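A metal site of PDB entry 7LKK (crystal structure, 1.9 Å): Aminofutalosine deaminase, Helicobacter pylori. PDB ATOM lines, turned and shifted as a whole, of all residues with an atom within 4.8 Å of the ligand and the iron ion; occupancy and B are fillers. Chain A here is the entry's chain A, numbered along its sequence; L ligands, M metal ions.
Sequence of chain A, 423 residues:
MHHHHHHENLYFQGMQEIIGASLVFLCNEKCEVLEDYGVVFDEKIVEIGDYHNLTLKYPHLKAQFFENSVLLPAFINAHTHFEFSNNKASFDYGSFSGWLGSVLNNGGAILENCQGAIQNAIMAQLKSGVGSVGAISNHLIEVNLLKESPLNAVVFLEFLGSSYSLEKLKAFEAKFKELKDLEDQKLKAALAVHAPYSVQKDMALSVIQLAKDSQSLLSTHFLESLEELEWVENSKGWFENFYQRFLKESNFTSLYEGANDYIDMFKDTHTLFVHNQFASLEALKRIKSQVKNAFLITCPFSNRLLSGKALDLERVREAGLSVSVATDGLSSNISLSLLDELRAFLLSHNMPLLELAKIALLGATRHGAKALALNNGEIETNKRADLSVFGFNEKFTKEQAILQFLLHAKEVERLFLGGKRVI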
ATOM      1  N   HIS A  79     -30.120 -19.067 -14.701  1.00  0.00           N
ATOM      2  CA  HIS A  79     -28.704 -19.114 -14.334  1.00  0.00           C
ATOM      3  C   HIS A  79     -27.918 -19.811 -15.440  1.00  0.00           C
ATOM      4  O   HIS A  79     -28.006 -21.037 -15.583  1.00  0.00           O
ATOM      5  CB  HIS A  79     -28.513 -19.827 -13.000  1.00  0.00           C
ATOM      6  CG  HIS A  79     -27.118 -19.767 -12.473  1.00  0.00           C
ATOM      7  ND1 HIS A  79     -26.636 -18.688 -11.765  1.00  0.00           N
ATOM      8  CD2 HIS A  79     -26.089 -20.654 -12.556  1.00  0.00           C
ATOM      9  CE1 HIS A  79     -25.379 -18.913 -11.428  1.00  0.00           C
ATOM     10  NE2 HIS A  79     -25.027 -20.089 -11.894  1.00  0.00           N
ATOM     11  N   HIS A  81     -23.935 -19.332 -17.804  1.00  0.00           N
ATOM     12  CA  HIS A  81     -22.655 -18.646 -18.022  1.00  0.00           C
ATOM     13  C   HIS A  81     -22.314 -18.731 -19.507  1.00  0.00           C
ATOM     14  O   HIS A  81     -21.666 -19.679 -19.947  1.00  0.00           O
ATOM     15  CB  HIS A  81     -21.531 -19.265 -17.169  1.00  0.00           C
ATOM     16  CG  HIS A  81     -21.809 -19.279 -15.707  1.00  0.00           C
ATOM     17  ND1 HIS A  81     -21.189 -18.431 -14.815  1.00  0.00           N
ATOM     18  CD2 HIS A  81     -22.639 -20.055 -14.960  1.00  0.00           C
ATOM     19  CE1 HIS A  81     -21.617 -18.678 -13.592  1.00  0.00           C
ATOM     20  NE2 HIS A  81     -22.501 -19.653 -13.649  1.00  0.00           N
ATOM     21  N   PHE A  84     -18.535 -19.108 -20.946  1.00  0.00           N
ATOM     22  CA  PHE A  84     -17.857 -20.402 -20.946  1.00  0.00           C
ATOM     23  C   PHE A  84     -18.403 -21.346 -22.004  1.00  0.00           C
ATOM     24  O   PHE A  84     -18.249 -22.567 -21.870  1.00  0.00           O
ATOM     25  CB  PHE A  84     -17.962 -21.047 -19.564  1.00  0.00           C
ATOM     26  CG  PHE A  84     -17.126 -20.376 -18.512  1.00  0.00           C
ATOM     27  CD1 PHE A  84     -15.798 -20.713 -18.334  1.00  0.00           C
ATOM     28  CD2 PHE A  84     -17.688 -19.415 -17.683  1.00  0.00           C
ATOM     29  CE1 PHE A  84     -15.038 -20.110 -17.354  1.00  0.00           C
ATOM     30  CE2 PHE A  84     -16.924 -18.796 -16.709  1.00  0.00           C
ATOM     31  CZ  PHE A  84     -15.599 -19.143 -16.544  1.00  0.00           C
ATOM     32  N   PHE A  96     -15.882 -31.336  -7.094  1.00  0.00           N
ATOM     33  CA  PHE A  96     -15.886 -29.889  -7.229  1.00  0.00           C
ATOM     34  C   PHE A  96     -14.463 -29.329  -7.185  1.00  0.00           C
ATOM     35  O   PHE A  96     -14.124 -28.443  -7.974  1.00  0.00           O
ATOM     36  CB  PHE A  96     -16.735 -29.239  -6.137  1.00  0.00           C
ATOM     37  CG  PHE A  96     -16.739 -27.739  -6.186  1.00  0.00           C
ATOM     38  CD1 PHE A  96     -17.640 -27.074  -7.000  1.00  0.00           C
ATOM     39  CD2 PHE A  96     -15.823 -27.005  -5.456  1.00  0.00           C
ATOM     40  CE1 PHE A  96     -17.643 -25.691  -7.058  1.00  0.00           C
ATOM     41  CE2 PHE A  96     -15.821 -25.631  -5.516  1.00  0.00           C
ATOM     42  CZ  PHE A  96     -16.731 -24.973  -6.322  1.00  0.00           C
ATOM     43  N   TRP A  99     -12.869 -29.887 -10.425  1.00  0.00           N
ATOM     44  CA  TRP A  99     -13.400 -28.992 -11.437  1.00  0.00           C
ATOM     45  C   TRP A  99     -12.843 -27.573 -11.271  1.00  0.00           C
ATOM     46  O   TRP A  99     -12.321 -26.992 -12.222  1.00  0.00           O
ATOM     47  CB  TRP A  99     -14.931 -28.982 -11.373  1.00  0.00           C
ATOM     48  CG  TRP A  99     -15.566 -28.009 -12.328  1.00  0.00           C
ATOM     49  CD1 TRP A  99     -15.839 -28.217 -13.647  1.00  0.00           C
ATOM     50  CD2 TRP A  99     -15.993 -26.673 -12.031  1.00  0.00           C
ATOM     51  NE1 TRP A  99     -16.421 -27.099 -14.193  1.00  0.00           N
ATOM     52  CE2 TRP A  99     -16.519 -26.131 -13.223  1.00  0.00           C
ATOM     53  CE3 TRP A  99     -15.976 -25.877 -10.883  1.00  0.00           C
ATOM     54  CZ2 TRP A  99     -17.040 -24.843 -13.291  1.00  0.00           C
ATOM     55  CZ3 TRP A  99     -16.491 -24.598 -10.953  1.00  0.00           C
ATOM     56  CH2 TRP A  99     -17.011 -24.088 -12.143  1.00  0.00           C
ATOM     57  N   LEU A 100     -12.936 -27.030 -10.056  1.00  0.00           N
ATOM     58  CA  LEU A 100     -12.496 -25.650  -9.831  1.00  0.00           C
ATOM     59  C   LEU A 100     -10.998 -25.502 -10.094  1.00  0.00           C
ATOM     60  O   LEU A 100     -10.573 -24.518 -10.710  1.00  0.00           O
ATOM     61  CB  LEU A 100     -12.843 -25.218  -8.405  1.00  0.00           C
ATOM     62  CG  LEU A 100     -12.519 -23.765  -8.032  1.00  0.00           C
ATOM     63  CD1 LEU A 100     -13.049 -22.799  -9.088  1.00  0.00           C
ATOM     64  CD2 LEU A 100     -13.072 -23.424  -6.667  1.00  0.00           C
ATOM     65  N   VAL A 103     -10.541 -25.322 -13.797  1.00  0.00           N
ATOM     66  CA  VAL A 103     -10.968 -24.046 -14.349  1.00  0.00           C
ATOM     67  C   VAL A 103      -9.887 -22.992 -14.143  1.00  0.00           C
ATOM     68  O   VAL A 103      -9.532 -22.237 -15.056  1.00  0.00           O
ATOM     69  CB  VAL A 103     -12.301 -23.608 -13.719  1.00  0.00           C
ATOM     70  CG1 VAL A 103     -12.645 -22.179 -14.127  1.00  0.00           C
ATOM     71  CG2 VAL A 103     -13.429 -24.560 -14.128  1.00  0.00           C
ATOM     72  N   LEU A 104      -9.327 -22.941 -12.925  1.00  0.00           N
ATOM     73  CA  LEU A 104      -8.290 -21.959 -12.635  1.00  0.00           C
ATOM     74  C   LEU A 104      -7.021 -22.258 -13.419  1.00  0.00           C
ATOM     75  O   LEU A 104      -6.393 -21.340 -13.973  1.00  0.00           O
ATOM     76  CB  LEU A 104      -8.012 -21.933 -11.134  1.00  0.00           C
ATOM     77  CG  LEU A 104      -9.151 -21.378 -10.272  1.00  0.00           C
ATOM     78  CD1 LEU A 104      -9.262 -22.130  -8.968  1.00  0.00           C
ATOM     79  CD2 LEU A 104      -8.954 -19.893 -10.019  1.00  0.00           C
ATOM     80  N   ILE A 136     -25.038 -14.918 -16.041  1.00  0.00           N
ATOM     81  CA  ILE A 136     -23.919 -14.532 -15.174  1.00  0.00           C
ATOM     82  C   ILE A 136     -22.743 -14.147 -16.049  1.00  0.00           C
ATOM     83  O   ILE A 136     -22.334 -14.890 -16.942  1.00  0.00           O
ATOM     84  CB  ILE A 136     -23.551 -15.673 -14.219  1.00  0.00           C
ATOM     85  CG1 ILE A 136     -24.769 -16.108 -13.400  1.00  0.00           C
ATOM     86  CG2 ILE A 136     -22.400 -15.252 -13.312  1.00  0.00           C
ATOM     87  CD1 ILE A 136     -24.989 -15.280 -12.149  1.00  0.00           C
ATOM     88  N   ASN A 138     -18.778 -12.148 -16.106  1.00  0.00           N
ATOM     89  CA  ASN A 138     -17.618 -11.568 -15.448  1.00  0.00           C
ATOM     90  C   ASN A 138     -16.979 -10.432 -16.246  1.00  0.00           C
ATOM     91  O   ASN A 138     -16.322  -9.577 -15.650  1.00  0.00           O
ATOM     92  CB  ASN A 138     -16.561 -12.648 -15.186  1.00  0.00           C
ATOM     93  CG  ASN A 138     -17.062 -13.737 -14.268  1.00  0.00           C
ATOM     94  OD1 ASN A 138     -17.043 -14.919 -14.623  1.00  0.00           O
ATOM     95  ND2 ASN A 138     -17.522 -13.357 -13.086  1.00  0.00           N
ATOM     96  N   GLU A 158     -20.906 -10.426 -12.265  1.00  0.00           N
ATOM     97  CA  GLU A 158     -20.487 -11.229 -11.120  1.00  0.00           C
ATOM     98  C   GLU A 158     -19.115 -10.779 -10.631  1.00  0.00           C
ATOM     99  O   GLU A 158     -18.171 -10.703 -11.426  1.00  0.00           O
ATOM    100  CB  GLU A 158     -20.454 -12.712 -11.489  1.00  0.00           C
ATOM    101  CG  GLU A 158     -19.891 -13.604 -10.403  1.00  0.00           C
ATOM    102  CD  GLU A 158     -19.844 -15.054 -10.824  1.00  0.00           C
ATOM    103  OE1 GLU A 158     -19.017 -15.395 -11.695  1.00  0.00           O
ATOM    104  OE2 GLU A 158     -20.647 -15.850 -10.287  1.00  0.00           O
ATOM    105  N   LEU A 160     -15.664 -11.178  -8.489  1.00  0.00           N
ATOM    106  CA  LEU A 160     -14.694 -12.132  -7.961  1.00  0.00           C
ATOM    107  C   LEU A 160     -13.595 -11.364  -7.248  1.00  0.00           C
ATOM    108  O   LEU A 160     -13.116 -10.347  -7.752  1.00  0.00           O
ATOM    109  CB  LEU A 160     -14.079 -12.997  -9.074  1.00  0.00           C
ATOM    110  CG  LEU A 160     -14.815 -14.206  -9.647  1.00  0.00           C
ATOM    111  CD1 LEU A 160     -14.817 -15.350  -8.644  1.00  0.00           C
ATOM    112  CD2 LEU A 160     -16.225 -13.883 -10.100  1.00  0.00           C
ATOM    113  N   HIS A 194     -19.846 -14.010  -6.275  1.00  0.00           N
ATOM    114  CA  HIS A 194     -19.568 -15.340  -6.803  1.00  0.00           C
ATOM    115  C   HIS A 194     -19.890 -16.423  -5.784  1.00  0.00           C
ATOM    116  O   HIS A 194     -20.756 -17.278  -6.006  1.00  0.00           O
ATOM    117  CB  HIS A 194     -18.124 -15.457  -7.267  1.00  0.00           C
ATOM    118  CG  HIS A 194     -17.778 -16.834  -7.763  1.00  0.00           C
ATOM    119  ND1 HIS A 194     -17.066 -17.736  -7.015  1.00  0.00           N
ATOM    120  CD2 HIS A 194     -18.104 -17.464  -8.911  1.00  0.00           C
ATOM    121  CE1 HIS A 194     -16.940 -18.864  -7.684  1.00  0.00           C
ATOM    122  NE2 HIS A 194     -17.562 -18.726  -8.846  1.00  0.00           N
ATOM    123  N   TYR A 197     -16.305 -18.568  -0.783  1.00  0.00           N
ATOM    124  CA  TYR A 197     -14.876 -18.831  -0.758  1.00  0.00           C
ATOM    125  C   TYR A 197     -14.081 -17.908  -1.666  1.00  0.00           C
ATOM    126  O   TYR A 197     -12.841 -17.903  -1.592  1.00  0.00           O
ATOM    127  CB  TYR A 197     -14.590 -20.291  -1.164  1.00  0.00           C
ATOM    128  CG  TYR A 197     -15.194 -20.693  -2.491  1.00  0.00           C
ATOM    129  CD1 TYR A 197     -14.611 -20.317  -3.697  1.00  0.00           C
ATOM    130  CD2 TYR A 197     -16.350 -21.469  -2.538  1.00  0.00           C
ATOM    131  CE1 TYR A 197     -15.161 -20.689  -4.902  1.00  0.00           C
ATOM    132  CE2 TYR A 197     -16.909 -21.846  -3.744  1.00  0.00           C
ATOM    133  CZ  TYR A 197     -16.306 -21.451  -4.925  1.00  0.00           C
ATOM    134  OH  TYR A 197     -16.869 -21.820  -6.129  1.00  0.00           O
ATOM    135  N   SER A 198     -14.737 -17.128  -2.516  1.00  0.00           N
ATOM    136  CA  SER A 198     -14.059 -16.350  -3.536  1.00  0.00           C
ATOM    137  C   SER A 198     -14.231 -14.838  -3.412  1.00  0.00           C
ATOM    138  O   SER A 198     -13.578 -14.102  -4.156  1.00  0.00           O
ATOM    139  CB  SER A 198     -14.532 -16.773  -4.936  1.00  0.00           C
ATOM    140  OG  SER A 198     -15.912 -16.533  -5.099  1.00  0.00           O
ATOM    141  N   HIS A 221     -23.604 -18.103  -5.752  1.00  0.00           N
ATOM    142  CA  HIS A 221     -23.436 -19.541  -5.579  1.00  0.00           C
ATOM    143  C   HIS A 221     -23.295 -19.839  -4.091  1.00  0.00           C
ATOM    144  O   HIS A 221     -22.501 -19.183  -3.406  1.00  0.00           O
ATOM    145  CB  HIS A 221     -22.220 -20.057  -6.346  1.00  0.00           C
ATOM    146  CG  HIS A 221     -22.268 -19.765  -7.812  1.00  0.00           C
ATOM    147  ND1 HIS A 221     -21.610 -18.694  -8.378  1.00  0.00           N
ATOM    148  CD2 HIS A 221     -22.879 -20.411  -8.829  1.00  0.00           C
ATOM    149  CE1 HIS A 221     -21.824 -18.687  -9.683  1.00  0.00           C
ATOM    150  NE2 HIS A 221     -22.583 -19.723  -9.977  1.00  0.00           N
ATOM    151  N   GLU A 224     -22.242 -25.257  -2.693  1.00  0.00           N
ATOM    152  CA  GLU A 224     -22.294 -26.130  -3.861  1.00  0.00           C
ATOM    153  C   GLU A 224     -21.483 -27.409  -3.667  1.00  0.00           C
ATOM    154  O   GLU A 224     -21.644 -28.353  -4.455  1.00  0.00           O
ATOM    155  CB  GLU A 224     -21.776 -25.360  -5.075  1.00  0.00           C
ATOM    156  CG  GLU A 224     -21.921 -26.062  -6.409  1.00  0.00           C
ATOM    157  CD  GLU A 224     -21.390 -25.215  -7.552  1.00  0.00           C
ATOM    158  OE1 GLU A 224     -20.864 -24.114  -7.290  1.00  0.00           O
ATOM    159  OE2 GLU A 224     -21.511 -25.654  -8.706  1.00  0.00           O
ATOM    160  N   HIS A 275     -27.605 -23.591  -6.431  1.00  0.00           N
ATOM    161  CA  HIS A 275     -27.082 -24.903  -6.039  1.00  0.00           C
ATOM    162  C   HIS A 275     -27.616 -25.334  -4.669  1.00  0.00           C
ATOM    163  O   HIS A 275     -28.660 -25.994  -4.601  1.00  0.00           O
ATOM    164  CB  HIS A 275     -25.557 -24.911  -6.071  1.00  0.00           C
ATOM    165  CG  HIS A 275     -24.988 -24.548  -7.415  1.00  0.00           C
ATOM    166  ND1 HIS A 275     -25.333 -25.225  -8.565  1.00  0.00           N
ATOM    167  CD2 HIS A 275     -24.130 -23.574  -7.793  1.00  0.00           C
ATOM    168  CE1 HIS A 275     -24.686 -24.692  -9.596  1.00  0.00           C
ATOM    169  NE2 HIS A 275     -23.960 -23.688  -9.146  1.00  0.00           N
ATOM    170  N   SER A 302     -25.083 -29.930 -13.626  1.00  0.00           N
ATOM    171  CA  SER A 302     -23.877 -29.365 -13.042  1.00  0.00           C
ATOM    172  C   SER A 302     -23.591 -29.956 -11.664  1.00  0.00           C
ATOM    173  O   SER A 302     -22.441 -30.292 -11.348  1.00  0.00           O
ATOM    174  CB  SER A 302     -23.989 -27.843 -12.956  1.00  0.00           C
ATOM    175  OG  SER A 302     -22.949 -27.295 -12.175  1.00  0.00           O
ATOM    176  N   LEU A 306     -20.086 -31.999 -10.713  1.00  0.00           N
ATOM    177  CA  LEU A 306     -19.125 -31.401  -9.789  1.00  0.00           C
ATOM    178  C   LEU A 306     -19.111 -32.150  -8.469  1.00  0.00           C
ATOM    179  O   LEU A 306     -18.404 -33.156  -8.335  1.00  0.00           O
ATOM    180  CB  LEU A 306     -19.452 -29.912  -9.573  1.00  0.00           C
ATOM    181  CG  LEU A 306     -18.747 -28.910 -10.496  1.00  0.00           C
ATOM    182  CD1 LEU A 306     -18.860 -29.311 -11.950  1.00  0.00           C
ATOM    183  CD2 LEU A 306     -19.297 -27.501 -10.277  1.00  0.00           C
ATOM    184  N   ASP A 328     -27.128 -23.880 -15.942  1.00  0.00           N
ATOM    185  CA  ASP A 328     -25.760 -23.422 -15.709  1.00  0.00           C
ATOM    186  C   ASP A 328     -25.108 -23.197 -17.064  1.00  0.00           C
ATOM    187  O   ASP A 328     -25.791 -23.023 -18.075  1.00  0.00           O
ATOM    188  CB  ASP A 328     -24.969 -24.427 -14.870  1.00  0.00           C
ATOM    189  CG  ASP A 328     -24.162 -23.761 -13.770  1.00  0.00           C
ATOM    190  OD1 ASP A 328     -23.969 -22.530 -13.838  1.00  0.00           O
ATOM    191  OD2 ASP A 328     -23.704 -24.465 -12.847  1.00  0.00           O
ATOM    192  N   SER A 331     -19.553 -24.810 -19.050  1.00  0.00           N
ATOM    193  CA  SER A 331     -18.446 -25.111 -18.159  1.00  0.00           C
ATOM    194  C   SER A 331     -18.774 -26.247 -17.195  1.00  0.00           C
ATOM    195  O   SER A 331     -17.853 -26.836 -16.610  1.00  0.00           O
ATOM    196  CB  SER A 331     -18.058 -23.859 -17.360  1.00  0.00           C
ATOM    197  OG  SER A 331     -19.211 -23.094 -17.033  1.00  0.00           O
ATOM    198  N   SER A 332     -20.062 -26.567 -17.020  1.00  0.00           N
ATOM    199  CA  SER A 332     -20.464 -27.639 -16.115  1.00  0.00           C
ATOM    200  C   SER A 332     -21.727 -28.328 -16.629  1.00  0.00           C
ATOM    201  O   SER A 332     -22.621 -28.680 -15.860  1.00  0.00           O
ATOM    202  CB  SER A 332     -20.687 -27.116 -14.693  1.00  0.00           C
ATOM    203  OG  SER A 332     -21.524 -25.968 -14.704  1.00  0.00           O
HETATM  204  O1  LIG L   1     -21.990 -22.092 -11.145  1.00  0.00           O
HETATM  205  C1  LIG L   1     -21.111 -22.928 -11.860  1.00  0.00           C
HETATM  206  C2  LIG L   1     -20.292 -23.825 -10.942  1.00  0.00           C
HETATM  207  N1  LIG L   1     -20.040 -23.186  -9.671  1.00  0.00           N
HETATM  208  C3  LIG L   1     -19.505 -21.843  -9.658  1.00  0.00           C
HETATM  209  N2  LIG L   1     -19.200 -21.024 -10.825  1.00  0.00           N
HETATM  210  C4  LIG L   1     -19.277 -21.245 -12.285  1.00  0.00           C
HETATM  211  C5  LIG L   1     -20.196 -22.135 -12.817  1.00  0.00           C
HETATM  212  N3  LIG L   1     -20.046 -22.127 -14.129  1.00  0.00           N
HETATM  213  C6  LIG L   1     -19.097 -21.260 -14.469  1.00  0.00           C
HETATM  214  N4  LIG L   1     -18.632 -20.720 -13.339  1.00  0.00           N
HETATM  215  C7  LIG L   1     -17.534 -19.699 -13.315  1.00  0.00           C
HETATM  216  C8  LIG L   1     -17.787 -18.528 -12.341  1.00  0.00           C
HETATM  217  O2  LIG L   1     -18.561 -17.569 -12.933  1.00  0.00           O
HETATM  218  O3  LIG L   1     -16.452 -20.238 -12.876  1.00  0.00           O
HETATM  219  C9  LIG L   1     -15.590 -19.024 -12.235  1.00  0.00           C
HETATM  220  C10 LIG L   1     -16.381 -18.002 -12.090  1.00  0.00           C
HETATM  221  O4  LIG L   1     -16.033 -16.960 -13.118  1.00  0.00           O
HETATM  222  C11 LIG L   1     -15.044 -19.467 -10.894  1.00  0.00           C
HETATM  223  S1  LIG L   1     -13.459 -18.629 -10.569  1.00  0.00           S
HETATM  224  C12 LIG L   1     -13.100 -18.689  -8.788  1.00  0.00           C
HETATM  225 FE    FE M   1     -23.068 -20.731 -12.070  1.00  0.00          FE
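O2 of the ligand is in hydrogen-bond range of OE1 of Glu 158. The side-chain carboxylate (OD1) of Asp 328 lies close to an oxygen (O1) of the ligand (3.4 Å). The side-chain carboxylate of Glu 224 sits at hydrogen-bond distance from a nitrogen (N1) of the ligand, 2.7 Å away. The side-chain amide oxygen (OD1) of Asn 138 is in hydrogen-bond range of an oxygen (O4) of the ligand. OG of Ser 331 sits close to N3 of the ligand. A ring nitrogen (NE2) of His 275 sits close to an oxygen (O1) of the ligand (3.2 Å). A ring nitrogen (NE2) of His 194 lies close to a nitrogen (N2) of the ligand (3.4 Å).
OD1 of Asp 328 lies close to NE2 of His 81. The backbone NH (N) of Asp 328 is in hydrogen-bond range of the backbone carbonyl oxygen (O) of His 79, 3.0 Å away. O of His 194 lies within hydrogen-bond range of ND1 of His 221 (2.9 Å). The side-chain carboxylate (OD2) of Asp 328 sits at hydrogen-bond distance from the side-chain hydroxyl (OG) of Ser 302 (3.0 Å). The side-chain carboxylate (OE2) of Glu 224 is in hydrogen-bond range of a ring nitrogen (NE2) of His 275, 3.2 Å away. The indole nitrogen (NE1) of Trp 99 sits at hydrogen-bond distance from the backbone carbonyl oxygen (O) of Ser 331, 2.8 Å away. ND1 of His 194 sits at hydrogen-bond distance from OG of Ser 198 (2.5 Å). The backbone NH of Phe 96 is in hydrogen-bond range of the backbone carbonyl oxygen of Leu 306 (3.3 Å).
The nearest printed residue that does not touch the iron ion is His 275 (4.3 Å).
Phe 84 touches the ligand (CE2 to C7, 3.6 Å). Trp 99 touches the ligand. CD1 of Leu 160 touches C12 of the ligand, at 3.8 Å. Leu 306 touches the ligand (CD2 to C2, 3.9 Å). Hydrophobic or aromatic side chains that line the ligand: His 81, Phe 84, Trp 99, Leu 160, His 194, His 221 and Leu 306. 14 residues have an atom within 4 Å of the ligand: His 79, His 81, Phe 84, Trp 99, Asn 138, Glu 158, Leu 160, His 194, His 221, Glu 224, His 275, Leu 306, Asp 328 and Ser 331. Along chain A the residues within 4 Å of the ligand span positions 79 to 331. The nearest printed residue that does not touch the ligand is Leu 100 (4.1 Å).
The iron ion is bound by O1 of the ligand (2.0 Å), NE2 of His 81 (2.0 Å), NE2 of His 79 (2.1 Å) and NE2 of His 221 (2.4 Å). The iron ion has four donor atoms within binding distance. Slightly farther from the iron ion lies OD1 of Asp 328 (2.7 Å).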
